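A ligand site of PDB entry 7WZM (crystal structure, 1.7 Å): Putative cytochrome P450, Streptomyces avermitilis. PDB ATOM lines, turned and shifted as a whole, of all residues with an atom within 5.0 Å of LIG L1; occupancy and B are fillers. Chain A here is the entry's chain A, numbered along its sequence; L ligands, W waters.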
ATOM      1  N   LEU A  85      -9.979  25.338 -16.953  1.00  0.00           N
ATOM      2  CA  LEU A  85     -10.432  24.252 -17.840  1.00  0.00           C
ATOM      3  C   LEU A  85     -11.653  23.560 -17.271  1.00  0.00           C
ATOM      4  O   LEU A  85     -12.352  22.942 -18.114  1.00  0.00           O
ATOM      5  CB  LEU A  85      -9.315  23.257 -18.077  1.00  0.00           C
ATOM      6  CG  LEU A  85      -8.135  23.760 -18.894  1.00  0.00           C
ATOM      7  CD1 LEU A  85      -7.090  22.646 -19.008  1.00  0.00           C
ATOM      8  CD2 LEU A  85      -8.506  24.260 -20.266  1.00  0.00           C
ATOM      9  N   LYS A  94     -13.710  29.098 -26.210  1.00  0.00           N
ATOM     10  CA  LYS A  94     -12.868  28.935 -27.407  1.00  0.00           C
ATOM     11  C   LYS A  94     -13.146  30.061 -28.406  1.00  0.00           C
ATOM     12  O   LYS A  94     -13.454  29.796 -29.601  1.00  0.00           O
ATOM     13  CB  LYS A  94     -13.034  27.540 -27.999  1.00  0.00           C
ATOM     14  CG  LYS A  94     -12.692  26.440 -26.997  1.00  0.00           C
ATOM     15  CD  LYS A  94     -12.808  25.125 -27.622  1.00  0.00           C
ATOM     16  CE  LYS A  94     -12.467  23.960 -26.731  1.00  0.00           C
ATOM     17  NZ  LYS A  94     -11.525  23.053 -27.409  1.00  0.00           N
ATOM     18  N   TYR A  99      -9.106  29.879 -33.240  1.00  0.00           N
ATOM     19  CA  TYR A  99     -10.187  28.863 -33.353  1.00  0.00           C
ATOM     20  C   TYR A  99     -11.003  29.151 -34.616  1.00  0.00           C
ATOM     21  O   TYR A  99     -11.444  28.210 -35.244  1.00  0.00           O
ATOM     22  CB  TYR A  99     -11.073  28.847 -32.105  1.00  0.00           C
ATOM     23  CG  TYR A  99     -10.402  28.179 -30.922  1.00  0.00           C
ATOM     24  CD1 TYR A  99     -10.088  26.835 -30.901  1.00  0.00           C
ATOM     25  CD2 TYR A  99     -10.139  28.905 -29.781  1.00  0.00           C
ATOM     26  CE1 TYR A  99      -9.504  26.263 -29.781  1.00  0.00           C
ATOM     27  CE2 TYR A  99      -9.540  28.359 -28.665  1.00  0.00           C
ATOM     28  CZ  TYR A  99      -9.217  27.029 -28.668  1.00  0.00           C
ATOM     29  OH  TYR A  99      -8.639  26.493 -27.553  1.00  0.00           O
ATOM     30  N   LEU A 110     -15.725  18.909 -33.382  1.00  0.00           N
ATOM     31  CA  LEU A 110     -15.908  18.707 -31.914  1.00  0.00           C
ATOM     32  C   LEU A 110     -14.921  19.630 -31.186  1.00  0.00           C
ATOM     33  O   LEU A 110     -15.202  20.003 -30.030  1.00  0.00           O
ATOM     34  CB  LEU A 110     -15.660  17.260 -31.526  1.00  0.00           C
ATOM     35  CG  LEU A 110     -16.118  16.888 -30.103  1.00  0.00           C
ATOM     36  CD1 LEU A 110     -17.662  16.927 -30.024  1.00  0.00           C
ATOM     37  CD2 LEU A 110     -15.637  15.491 -29.769  1.00  0.00           C
ATOM     38  N   LEU A 111     -13.741  19.872 -31.752  1.00  0.00           N
ATOM     39  CA  LEU A 111     -12.727  20.651 -30.987  1.00  0.00           C
ATOM     40  C   LEU A 111     -13.091  22.133 -30.912  1.00  0.00           C
ATOM     41  O   LEU A 111     -12.703  22.808 -29.911  1.00  0.00           O
ATOM     42  CB  LEU A 111     -11.348  20.475 -31.636  1.00  0.00           C
ATOM     43  CG  LEU A 111     -10.217  20.913 -30.708  1.00  0.00           C
ATOM     44  CD1 LEU A 111      -9.152  19.841 -30.583  1.00  0.00           C
ATOM     45  CD2 LEU A 111      -9.681  22.191 -31.247  1.00  0.00           C
ATOM     46  N   TYR A 118     -22.089  22.364 -30.017  1.00  0.00           N
ATOM     47  CA  TYR A 118     -21.188  21.413 -29.325  1.00  0.00           C
ATOM     48  C   TYR A 118     -21.966  20.325 -28.609  1.00  0.00           C
ATOM     49  O   TYR A 118     -21.611  19.135 -28.799  1.00  0.00           O
ATOM     50  CB  TYR A 118     -20.233  22.127 -28.365  1.00  0.00           C
ATOM     51  CG  TYR A 118     -19.387  21.133 -27.645  1.00  0.00           C
ATOM     52  CD1 TYR A 118     -18.279  20.547 -28.257  1.00  0.00           C
ATOM     53  CD2 TYR A 118     -19.778  20.655 -26.392  1.00  0.00           C
ATOM     54  CE1 TYR A 118     -17.562  19.577 -27.621  1.00  0.00           C
ATOM     55  CE2 TYR A 118     -19.055  19.679 -25.746  1.00  0.00           C
ATOM     56  CZ  TYR A 118     -17.922  19.149 -26.352  1.00  0.00           C
ATOM     57  OH  TYR A 118     -17.188  18.164 -25.707  1.00  0.00           O
ATOM     58  N   ARG A 122     -21.426  16.374 -29.197  1.00  0.00           N
ATOM     59  CA  ARG A 122     -20.917  15.516 -28.089  1.00  0.00           C
ATOM     60  C   ARG A 122     -21.849  14.330 -27.866  1.00  0.00           C
ATOM     61  O   ARG A 122     -21.396  13.231 -27.686  1.00  0.00           O
ATOM     62  CB  ARG A 122     -20.769  16.368 -26.821  1.00  0.00           C
ATOM     63  CG  ARG A 122     -20.203  15.609 -25.634  1.00  0.00           C
ATOM     64  CD  ARG A 122     -18.737  15.216 -25.705  1.00  0.00           C
ATOM     65  NE  ARG A 122     -18.394  14.620 -24.435  1.00  0.00           N
ATOM     66  CZ  ARG A 122     -17.918  15.286 -23.381  1.00  0.00           C
ATOM     67  NH1 ARG A 122     -17.709  16.583 -23.462  1.00  0.00           N
ATOM     68  NH2 ARG A 122     -17.655  14.643 -22.266  1.00  0.00           N
ATOM     69  N   PHE A 129     -16.639   6.654 -28.629  1.00  0.00           N
ATOM     70  CA  PHE A 129     -15.340   6.675 -27.915  1.00  0.00           C
ATOM     71  C   PHE A 129     -15.526   6.056 -26.519  1.00  0.00           C
ATOM     72  O   PHE A 129     -14.759   6.375 -25.579  1.00  0.00           O
ATOM     73  CB  PHE A 129     -14.817   8.109 -27.821  1.00  0.00           C
ATOM     74  CG  PHE A 129     -14.268   8.629 -29.124  1.00  0.00           C
ATOM     75  CD1 PHE A 129     -15.098   9.247 -30.031  1.00  0.00           C
ATOM     76  CD2 PHE A 129     -12.921   8.515 -29.432  1.00  0.00           C
ATOM     77  CE1 PHE A 129     -14.609   9.746 -31.223  1.00  0.00           C
ATOM     78  CE2 PHE A 129     -12.432   8.975 -30.634  1.00  0.00           C
ATOM     79  CZ  PHE A 129     -13.262   9.561 -31.547  1.00  0.00           C
ATOM     80  N   ILE A 284     -11.423  16.707 -38.035  1.00  0.00           N
ATOM     81  CA  ILE A 284     -10.872  17.058 -36.685  1.00  0.00           C
ATOM     82  C   ILE A 284     -10.262  15.833 -36.019  1.00  0.00           C
ATOM     83  O   ILE A 284      -9.277  15.973 -35.343  1.00  0.00           O
ATOM     84  CB  ILE A 284     -11.878  17.817 -35.788  1.00  0.00           C
ATOM     85  CG1 ILE A 284     -11.157  18.579 -34.682  1.00  0.00           C
ATOM     86  CG2 ILE A 284     -12.942  16.897 -35.217  1.00  0.00           C
ATOM     87  CD1 ILE A 284     -10.201  19.640 -35.175  1.00  0.00           C
ATOM     88  N   PHE A 285     -10.805  14.634 -36.275  1.00  0.00           N
ATOM     89  CA  PHE A 285     -10.170  13.414 -35.718  1.00  0.00           C
ATOM     90  C   PHE A 285      -8.755  13.245 -36.312  1.00  0.00           C
ATOM     91  O   PHE A 285      -7.826  12.933 -35.592  1.00  0.00           O
ATOM     92  CB  PHE A 285     -11.024  12.174 -35.971  1.00  0.00           C
ATOM     93  CG  PHE A 285     -12.377  12.177 -35.292  1.00  0.00           C
ATOM     94  CD1 PHE A 285     -12.670  13.071 -34.277  1.00  0.00           C
ATOM     95  CD2 PHE A 285     -13.348  11.272 -35.675  1.00  0.00           C
ATOM     96  CE1 PHE A 285     -13.922  13.079 -33.678  1.00  0.00           C
ATOM     97  CE2 PHE A 285     -14.587  11.269 -35.053  1.00  0.00           C
ATOM     98  CZ  PHE A 285     -14.870  12.169 -34.068  1.00  0.00           C
ATOM     99  N   ALA A 288      -6.609  16.359 -34.931  1.00  0.00           N
ATOM    100  CA  ALA A 288      -6.363  16.285 -33.481  1.00  0.00           C
ATOM    101  C   ALA A 288      -5.609  15.013 -33.104  1.00  0.00           C
ATOM    102  O   ALA A 288      -5.009  15.009 -32.038  1.00  0.00           O
ATOM    103  CB  ALA A 288      -7.664  16.392 -32.734  1.00  0.00           C
ATOM    104  N   GLY A 289      -5.700  13.969 -33.926  1.00  0.00           N
ATOM    105  CA  GLY A 289      -5.096  12.688 -33.514  1.00  0.00           C
ATOM    106  C   GLY A 289      -3.780  12.348 -34.208  1.00  0.00           C
ATOM    107  O   GLY A 289      -3.120  11.426 -33.773  1.00  0.00           O
ATOM    108  N   THR A 292      -0.287  14.973 -32.659  1.00  0.00           N
ATOM    109  CA  THR A 292      -0.252  14.868 -31.185  1.00  0.00           C
ATOM    110  C   THR A 292       0.365  13.528 -30.766  1.00  0.00           C
ATOM    111  O   THR A 292       1.320  13.508 -30.012  1.00  0.00           O
ATOM    112  CB  THR A 292      -1.689  15.040 -30.683  1.00  0.00           C
ATOM    113  OG1 THR A 292      -2.523  14.186 -31.471  1.00  0.00           O
ATOM    114  CG2 THR A 292      -2.169  16.475 -30.752  1.00  0.00           C
ATOM    115  N   THR A 293      -0.225  12.431 -31.237  1.00  0.00           N
ATOM    116  CA  THR A 293       0.279  11.092 -30.860  1.00  0.00           C
ATOM    117  C   THR A 293       1.697  10.897 -31.406  1.00  0.00           C
ATOM    118  O   THR A 293       2.514  10.340 -30.736  1.00  0.00           O
ATOM    119  CB  THR A 293      -0.686   9.974 -31.291  1.00  0.00           C
ATOM    120  OG1 THR A 293      -1.990  10.405 -30.929  1.00  0.00           O
ATOM    121  CG2 THR A 293      -0.389   8.646 -30.633  1.00  0.00           C
ATOM    122  N   ALA A 296       4.259  12.335 -29.025  1.00  0.00           N
ATOM    123  CA  ALA A 296       4.410  11.514 -27.813  1.00  0.00           C
ATOM    124  C   ALA A 296       5.221  10.258 -28.123  1.00  0.00           C
ATOM    125  O   ALA A 296       6.089   9.924 -27.353  1.00  0.00           O
ATOM    126  CB  ALA A 296       3.080  11.153 -27.239  1.00  0.00           C
ATOM    127  N   MET A 349       5.100  12.490 -22.104  1.00  0.00           N
ATOM    128  CA  MET A 349       4.133  13.594 -22.356  1.00  0.00           C
ATOM    129  C   MET A 349       4.264  14.717 -21.314  1.00  0.00           C
ATOM    130  O   MET A 349       3.944  15.862 -21.600  1.00  0.00           O
ATOM    131  CB  MET A 349       2.705  13.071 -22.400  1.00  0.00           C
ATOM    132  CG  MET A 349       2.510  12.124 -23.522  1.00  0.00           C
ATOM    133  SD  MET A 349       0.743  11.671 -23.605  1.00  0.00           S
ATOM    134  CE  MET A 349       0.726  10.391 -22.394  1.00  0.00           C
ATOM    135  N   SER A 354       2.372  17.531 -26.330  1.00  0.00           N
ATOM    136  CA  SER A 354       2.039  17.878 -27.728  1.00  0.00           C
ATOM    137  C   SER A 354       1.227  19.172 -27.822  1.00  0.00           C
ATOM    138  O   SER A 354       1.294  19.839 -28.907  1.00  0.00           O
ATOM    139  CB  SER A 354       1.336  16.770 -28.407  1.00  0.00           C
ATOM    140  OG  SER A 354       2.102  15.547 -28.410  1.00  0.00           O
ATOM    141  N   ALA A 355       0.437  19.520 -26.766  1.00  0.00           N
ATOM    142  CA  ALA A 355      -0.270  20.800 -26.670  1.00  0.00           C
ATOM    143  C   ALA A 355       0.371  21.606 -25.532  1.00  0.00           C
ATOM    144  O   ALA A 355       0.035  21.430 -24.363  1.00  0.00           O
ATOM    145  CB  ALA A 355      -1.745  20.575 -26.389  1.00  0.00           C
ATOM    146  N   ILE A 358      -2.809  25.853 -24.087  1.00  0.00           N
ATOM    147  CA  ILE A 358      -4.228  25.644 -24.456  1.00  0.00           C
ATOM    148  C   ILE A 358      -4.884  27.029 -24.292  1.00  0.00           C
ATOM    149  O   ILE A 358      -4.833  27.548 -23.205  1.00  0.00           O
ATOM    150  CB  ILE A 358      -4.908  24.571 -23.584  1.00  0.00           C
ATOM    151  CG1 ILE A 358      -4.181  23.226 -23.662  1.00  0.00           C
ATOM    152  CG2 ILE A 358      -6.385  24.450 -23.913  1.00  0.00           C
ATOM    153  CD1 ILE A 358      -4.588  22.243 -22.597  1.00  0.00           C
ATOM    154  N   ARG A 360      -7.780  30.219 -24.300  1.00  0.00           N
ATOM    155  CA  ARG A 360      -9.207  30.439 -24.010  1.00  0.00           C
ATOM    156  C   ARG A 360      -9.393  31.939 -24.087  1.00  0.00           C
ATOM    157  O   ARG A 360      -8.391  32.642 -24.272  1.00  0.00           O
ATOM    158  CB  ARG A 360      -9.604  29.978 -22.603  1.00  0.00           C
ATOM    159  CG  ARG A 360      -9.716  28.475 -22.422  1.00  0.00           C
ATOM    160  CD  ARG A 360     -10.752  27.830 -23.311  1.00  0.00           C
ATOM    161  NE  ARG A 360     -11.040  26.450 -22.944  1.00  0.00           N
ATOM    162  CZ  ARG A 360     -10.544  25.392 -23.563  1.00  0.00           C
ATOM    163  NH1 ARG A 360      -9.701  25.550 -24.574  1.00  0.00           N
ATOM    164  NH2 ARG A 360     -10.870  24.174 -23.164  1.00  0.00           N
ATOM    165  N   PRO A 419      -1.638  16.789 -20.133  1.00  0.00           N
ATOM    166  CA  PRO A 419      -1.351  16.926 -21.551  1.00  0.00           C
ATOM    167  C   PRO A 419      -2.594  16.777 -22.439  1.00  0.00           C
ATOM    168  O   PRO A 419      -2.547  17.249 -23.547  1.00  0.00           O
ATOM    169  CB  PRO A 419      -0.348  15.821 -21.858  1.00  0.00           C
ATOM    170  CG  PRO A 419      -0.620  14.776 -20.803  1.00  0.00           C
ATOM    171  CD  PRO A 419      -0.993  15.608 -19.562  1.00  0.00           C
ATOM    172  N   PHE A 420      -3.648  16.156 -21.911  1.00  0.00           N
ATOM    173  CA  PHE A 420      -4.933  15.963 -22.621  1.00  0.00           C
ATOM    174  C   PHE A 420      -5.958  16.973 -22.146  1.00  0.00           C
ATOM    175  O   PHE A 420      -7.154  16.788 -22.416  1.00  0.00           O
ATOM    176  CB  PHE A 420      -5.454  14.551 -22.360  1.00  0.00           C
ATOM    177  CG  PHE A 420      -4.588  13.450 -22.924  1.00  0.00           C
ATOM    178  CD1 PHE A 420      -4.604  13.160 -24.279  1.00  0.00           C
ATOM    179  CD2 PHE A 420      -3.692  12.784 -22.105  1.00  0.00           C
ATOM    180  CE1 PHE A 420      -3.807  12.164 -24.796  1.00  0.00           C
ATOM    181  CE2 PHE A 420      -2.932  11.758 -22.617  1.00  0.00           C
ATOM    182  CZ  PHE A 420      -2.975  11.447 -23.958  1.00  0.00           C
ATOM    183  N   GLY A 421      -5.531  18.008 -21.419  1.00  0.00           N
ATOM    184  CA  GLY A 421      -6.515  18.959 -20.890  1.00  0.00           C
ATOM    185  C   GLY A 421      -7.258  18.380 -19.720  1.00  0.00           C
ATOM    186  O   GLY A 421      -6.715  17.496 -18.979  1.00  0.00           O
ATOM    187  N   PRO A 424     -14.681  19.609 -18.997  1.00  0.00           N
ATOM    188  CA  PRO A 424     -15.746  19.244 -19.943  1.00  0.00           C
ATOM    189  C   PRO A 424     -15.265  19.112 -21.382  1.00  0.00           C
ATOM    190  O   PRO A 424     -16.008  18.544 -22.177  1.00  0.00           O
ATOM    191  CB  PRO A 424     -16.783  20.369 -19.783  1.00  0.00           C
ATOM    192  CG  PRO A 424     -16.053  21.489 -19.185  1.00  0.00           C
ATOM    193  CD  PRO A 424     -14.984  20.860 -18.303  1.00  0.00           C
ATOM    194  N   ARG A 425     -14.103  19.709 -21.701  1.00  0.00           N
ATOM    195  CA  ARG A 425     -13.599  19.730 -23.103  1.00  0.00           C
ATOM    196  C   ARG A 425     -12.254  18.983 -23.195  1.00  0.00           C
ATOM    197  O   ARG A 425     -11.501  19.236 -24.100  1.00  0.00           O
ATOM    198  CB  ARG A 425     -13.534  21.148 -23.680  1.00  0.00           C
ATOM    199  CG  ARG A 425     -14.833  21.915 -23.597  1.00  0.00           C
ATOM    200  CD  ARG A 425     -15.885  21.364 -24.536  1.00  0.00           C
ATOM    201  NE  ARG A 425     -15.426  21.325 -25.917  1.00  0.00           N
ATOM    202  CZ  ARG A 425     -15.738  22.225 -26.840  1.00  0.00           C
ATOM    203  NH1 ARG A 425     -16.538  23.234 -26.536  1.00  0.00           N
ATOM    204  NH2 ARG A 425     -15.283  22.091 -28.071  1.00  0.00           N
ATOM    205  N   ALA A 426     -12.035  18.084 -22.245  1.00  0.00           N
ATOM    206  CA  ALA A 426     -10.814  17.266 -22.267  1.00  0.00           C
ATOM    207  C   ALA A 426     -10.789  16.387 -23.521  1.00  0.00           C
ATOM    208  O   ALA A 426     -11.822  16.105 -24.090  1.00  0.00           O
ATOM    209  CB  ALA A 426     -10.779  16.387 -21.071  1.00  0.00           C
ATOM    210  N   CYS A 427      -9.597  15.944 -23.836  1.00  0.00           N
ATOM    211  CA  CYS A 427      -9.425  15.119 -25.039  1.00  0.00           C
ATOM    212  C   CYS A 427     -10.335  13.874 -25.061  1.00  0.00           C
ATOM    213  O   CYS A 427     -10.214  13.048 -24.179  1.00  0.00           O
ATOM    214  CB  CYS A 427      -8.005  14.628 -25.063  1.00  0.00           C
ATOM    215  SG  CYS A 427      -7.679  13.690 -26.578  1.00  0.00           S
ATOM    216  N   ILE A 428     -11.220  13.782 -26.060  1.00  0.00           N
ATOM    217  CA  ILE A 428     -12.091  12.577 -26.189  1.00  0.00           C
ATOM    218  C   ILE A 428     -11.259  11.383 -26.674  1.00  0.00           C
ATOM    219  O   ILE A 428     -11.638  10.258 -26.412  1.00  0.00           O
ATOM    220  CB  ILE A 428     -13.259  12.885 -27.149  1.00  0.00           C
ATOM    221  CG1 ILE A 428     -14.391  11.859 -27.043  1.00  0.00           C
ATOM    222  CG2 ILE A 428     -12.778  13.022 -28.578  1.00  0.00           C
ATOM    223  CD1 ILE A 428     -15.598  12.215 -27.868  1.00  0.00           C
ATOM    224  N   GLY A 429     -10.126  11.682 -27.311  1.00  0.00           N
ATOM    225  CA  GLY A 429      -9.223  10.634 -27.843  1.00  0.00           C
ATOM    226  C   GLY A 429      -8.123  10.191 -26.877  1.00  0.00           C
ATOM    227  O   GLY A 429      -7.255   9.384 -27.331  1.00  0.00           O
ATOM    228  N   LEU A 432      -7.830   6.286 -26.669  1.00  0.00           N
ATOM    229  CA  LEU A 432      -7.378   5.827 -28.016  1.00  0.00           C
ATOM    230  C   LEU A 432      -5.871   6.098 -28.186  1.00  0.00           C
ATOM    231  O   LEU A 432      -5.162   5.218 -28.596  1.00  0.00           O
ATOM    232  CB  LEU A 432      -8.191   6.535 -29.107  1.00  0.00           C
ATOM    233  CG  LEU A 432      -7.847   6.175 -30.548  1.00  0.00           C
ATOM    234  CD1 LEU A 432      -8.019   4.693 -30.791  1.00  0.00           C
ATOM    235  CD2 LEU A 432      -8.706   6.977 -31.506  1.00  0.00           C
ATOM    236  N   SER A 433      -5.455   7.306 -27.862  1.00  0.00           N
ATOM    237  CA  SER A 433      -4.024   7.688 -27.997  1.00  0.00           C
ATOM    238  C   SER A 433      -3.163   6.739 -27.148  1.00  0.00           C
ATOM    239  O   SER A 433      -2.079   6.394 -27.556  1.00  0.00           O
ATOM    240  CB  SER A 433      -3.751   9.119 -27.623  1.00  0.00           C
ATOM    241  OG  SER A 433      -3.583   9.252 -26.229  1.00  0.00           O
HETATM  242  C1  LIG L   1      -9.085  17.610 -27.348  1.00  0.00           C
HETATM  243  C2  LIG L   1      -4.404  16.685 -26.516  1.00  0.00           C
HETATM  244  C3  LIG L   1      -4.789  12.527 -29.049  1.00  0.00           C
HETATM  245  C4  LIG L   1      -9.085  14.075 -30.626  1.00  0.00           C
HETATM  246  C5  LIG L   1      -7.796  17.674 -26.881  1.00  0.00           C
HETATM  247  C6  LIG L   1      -7.333  18.625 -25.934  1.00  0.00           C
HETATM  248  C7  LIG L   1      -6.034  18.358 -25.717  1.00  0.00           C
HETATM  249  C8  LIG L   1      -5.658  17.250 -26.495  1.00  0.00           C
HETATM  250  C9  LIG L   1      -5.090  19.111 -24.811  1.00  0.00           C
HETATM  251  C10 LIG L   1      -8.123  19.738 -25.274  1.00  0.00           C
HETATM  252  C11 LIG L   1      -8.088  21.045 -26.048  1.00  0.00           C
HETATM  253  C12 LIG L   1      -8.864  22.160 -25.369  1.00  0.00           C
HETATM  254  O1  LIG L   1      -9.044  23.213 -26.007  1.00  0.00           O
HETATM  255  O2  LIG L   1      -9.332  22.035 -24.232  1.00  0.00           O
HETATM  256  C13 LIG L   1      -4.136  15.446 -27.132  1.00  0.00           C
HETATM  257  C14 LIG L   1      -2.865  14.805 -27.032  1.00  0.00           C
HETATM  258  C15 LIG L   1      -2.954  13.636 -27.731  1.00  0.00           C
HETATM  259  C16 LIG L   1      -4.321  13.588 -28.280  1.00  0.00           C
HETATM  260  C17 LIG L   1      -1.703  15.367 -26.264  1.00  0.00           C
HETATM  261  C18 LIG L   1      -1.965  12.570 -27.985  1.00  0.00           C
HETATM  262  C19 LIG L   1      -1.013  12.152 -27.171  1.00  0.00           C
HETATM  263  C20 LIG L   1      -6.003  12.569 -29.717  1.00  0.00           C
HETATM  264  C21 LIG L   1      -6.511  11.574 -30.573  1.00  0.00           C
HETATM  265  C22 LIG L   1      -7.750  12.018 -31.018  1.00  0.00           C
HETATM  266  C23 LIG L   1      -7.987  13.284 -30.424  1.00  0.00           C
HETATM  267  C24 LIG L   1      -5.836  10.285 -30.929  1.00  0.00           C
HETATM  268  C25 LIG L   1      -8.604  11.266 -31.974  1.00  0.00           C
HETATM  269  C26 LIG L   1      -9.926  11.316 -31.986  1.00  0.00           C
HETATM  270  C27 LIG L   1      -9.431  15.156 -29.815  1.00  0.00           C
HETATM  271  C28 LIG L   1     -10.723  15.846 -29.967  1.00  0.00           C
HETATM  272  C29 LIG L   1     -10.732  16.821 -29.053  1.00  0.00           C
HETATM  273  C30 LIG L   1      -9.427  16.725 -28.356  1.00  0.00           C
HETATM  274  C31 LIG L   1     -11.820  15.518 -30.965  1.00  0.00           C
HETATM  275  C32 LIG L   1     -11.858  17.778 -28.769  1.00  0.00           C
HETATM  276  C33 LIG L   1     -12.650  17.214 -27.572  1.00  0.00           C
HETATM  277  C34 LIG L   1     -13.838  18.037 -27.133  1.00  0.00           C
HETATM  278  O3  LIG L   1     -14.815  17.461 -26.634  1.00  0.00           O
HETATM  279  O4  LIG L   1     -13.828  19.273 -27.240  1.00  0.00           O
HETATM  280  N1  LIG L   1      -6.754  16.841 -27.198  1.00  0.00           N
HETATM  281  N2  LIG L   1      -4.947  14.690 -27.867  1.00  0.00           N
HETATM  282  N3  LIG L   1      -6.905  13.573 -29.649  1.00  0.00           N
HETATM  283  N4  LIG L   1      -8.706  15.721 -28.871  1.00  0.00           N
HETATM  284 FE1  LIG L   1      -6.967  15.185 -28.301  1.00  0.00          FE
HETATM  285  C1  LG2 L   2      -1.520  18.803 -33.695  1.00  0.00           C
HETATM  286  O1  LG2 L   2      -0.973  19.233 -32.762  1.00  0.00           O
HETATM  287  O2  LG2 L   2      -1.012  18.749 -34.810  1.00  0.00           O
HETATM  288  C2  LG2 L   2      -2.903  18.356 -33.434  1.00  0.00           C
HETATM  289  C3  LG2 L   2      -3.811  19.438 -33.907  1.00  0.00           C
HETATM  290  C4  LG2 L   2      -4.884  19.889 -32.958  1.00  0.00           C
HETATM  291  C5  LG2 L   2      -4.718  21.389 -32.853  1.00  0.00           C
HETATM  292  C6  LG2 L   2      -4.220  21.719 -31.474  1.00  0.00           C
HETATM  293  C7  LG2 L   2      -2.927  21.043 -31.033  1.00  0.00           C
HETATM  294  C8  LG2 L   2      -2.877  19.934 -29.978  1.00  0.00           C
HETATM  295  C9  LG2 L   2      -4.126  19.115 -29.747  1.00  0.00           C
HETATM  296  C10 LG2 L   2      -5.289  19.411 -29.179  1.00  0.00           C
HETATM  297  C11 LG2 L   2      -5.729  20.730 -28.630  1.00  0.00           C
HETATM  298  C12 LG2 L   2      -4.823  21.334 -27.582  1.00  0.00           C
HETATM  299  C13 LG2 L   2      -3.969  22.474 -28.130  1.00  0.00           C
HETATM  300  C14 LG2 L   2      -4.261  23.701 -27.347  1.00  0.00           C
HETATM  301  C15 LG2 L   2      -4.358  24.956 -28.153  1.00  0.00           C
HETATM  302  C16 LG2 L   2      -5.739  25.478 -27.950  1.00  0.00           C
HETATM  303  C17 LG2 L   2      -6.661  24.319 -27.587  1.00  0.00           C
HETATM  304  C18 LG2 L   2      -7.520  23.756 -28.702  1.00  0.00           C
HETATM  305  O   HOH W   1      -5.998  16.498 -29.860  1.00  0.00           O
HETATM  306  O   HOH W   2      -9.529  20.655 -21.760  1.00  0.00           O
HETATM  307  O   HOH W   3     -11.565  20.440 -26.566  1.00  0.00           O
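An oxygen (O3) of LIG L1 is in hydrogen-bond range of the side-chain hydroxyl (OH) of Tyr 118 (2.6 Å). An oxygen (O1) of LIG L1 lies within salt-bridge range of the guanidinium group (NH1) of Arg 360. The side-chain amino group (NZ) of Lys 94 lies within salt-bridge range of an oxygen (O1) of LIG L1. The guanidinium group of Arg 425 lies within salt-bridge range of an oxygen (O4) of LIG L1. FE1 of LIG L1 is bound by SG of Cys 427, at 2.4 Å.
O of Thr 292 lies within hydrogen-bond range of OG of Ser 354, 2.7 Å away. The side-chain amino group (NZ) of Lys 94 is in hydrogen-bond range of the backbone carbonyl oxygen (O) of Leu 111 (2.8 Å). OH of Tyr 118 is in hydrogen-bond range of NH1 of Arg 122 (2.8 Å). NH2 of Arg 425 lies within hydrogen-bond range of O of Leu 111 (3.2 Å). The backbone carbonyl oxygen (O) of Gly 289 lies within hydrogen-bond range of the side-chain hydroxyl (OG1) of Thr 293 (3.2 Å). The guanidinium group (NH2) of Arg 425 is in hydrogen-bond range of the backbone carbonyl oxygen (O) of Leu 110. O of Ala 288 is in hydrogen-bond range of OG1 of Thr 292. SG of Cys 427 sits close to N of Gly 429, at 3.2 Å.
O4 of LIG L1 lies close to O of Leu 110 (3.2 Å). O of Ala 288 lies close to N3 of LIG L1 (3.4 Å). Residues that only touch LIG L1: Phe 420 (3.4 Å), Pro 419 (3.4 Å), Gly 289 (3.4 Å), Thr 292 (3.5 Å), Ile 428 (3.6 Å), Gly 421 (3.6 Å), Ile 358 (3.6 Å), Tyr 99 (3.6 Å), Thr 293 (3.7 Å), Phe 129 (3.7 Å), Leu 111 (3.7 Å), Ala 426 (3.7 Å), Gly 429 (3.8 Å), Ser 433 (3.8 Å), Ser 354 (3.97 Å), Ala 355 (3.98 Å) and Phe 285 (3.98 Å). Hydrophobic or aromatic side chains that line LIG L1: Leu 110, Leu 111, Tyr 118, Phe 129, Phe 285, Ala 288, Ala 355, Ile 358, Phe 420 and Ile 428. 24 residues have an atom within 4 Å of LIG L1: Lys 94, Tyr 99, Leu 110, Leu 111, Tyr 118, Phe 129, Phe 285, Ala 288, Gly 289, Thr 292, Thr 293, Ser 354, Ala 355, Ile 358, Arg 360, Pro 419, Phe 420, Gly 421, Arg 425, Ala 426, Cys 427, Ile 428, Gly 429 and Ser 433.
Water W3 lies within hydrogen-bond range of an oxygen (O4) of LIG L1 (2.6 Å), the backbone carbonyl oxygen of Arg 425 (2.7 Å) and the side-chain amino group of Lys 94 (2.7 Å). Water W2 bridges O2 of LIG L1 (2.8 Å) and O of Arg 425 (3.4 Å).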
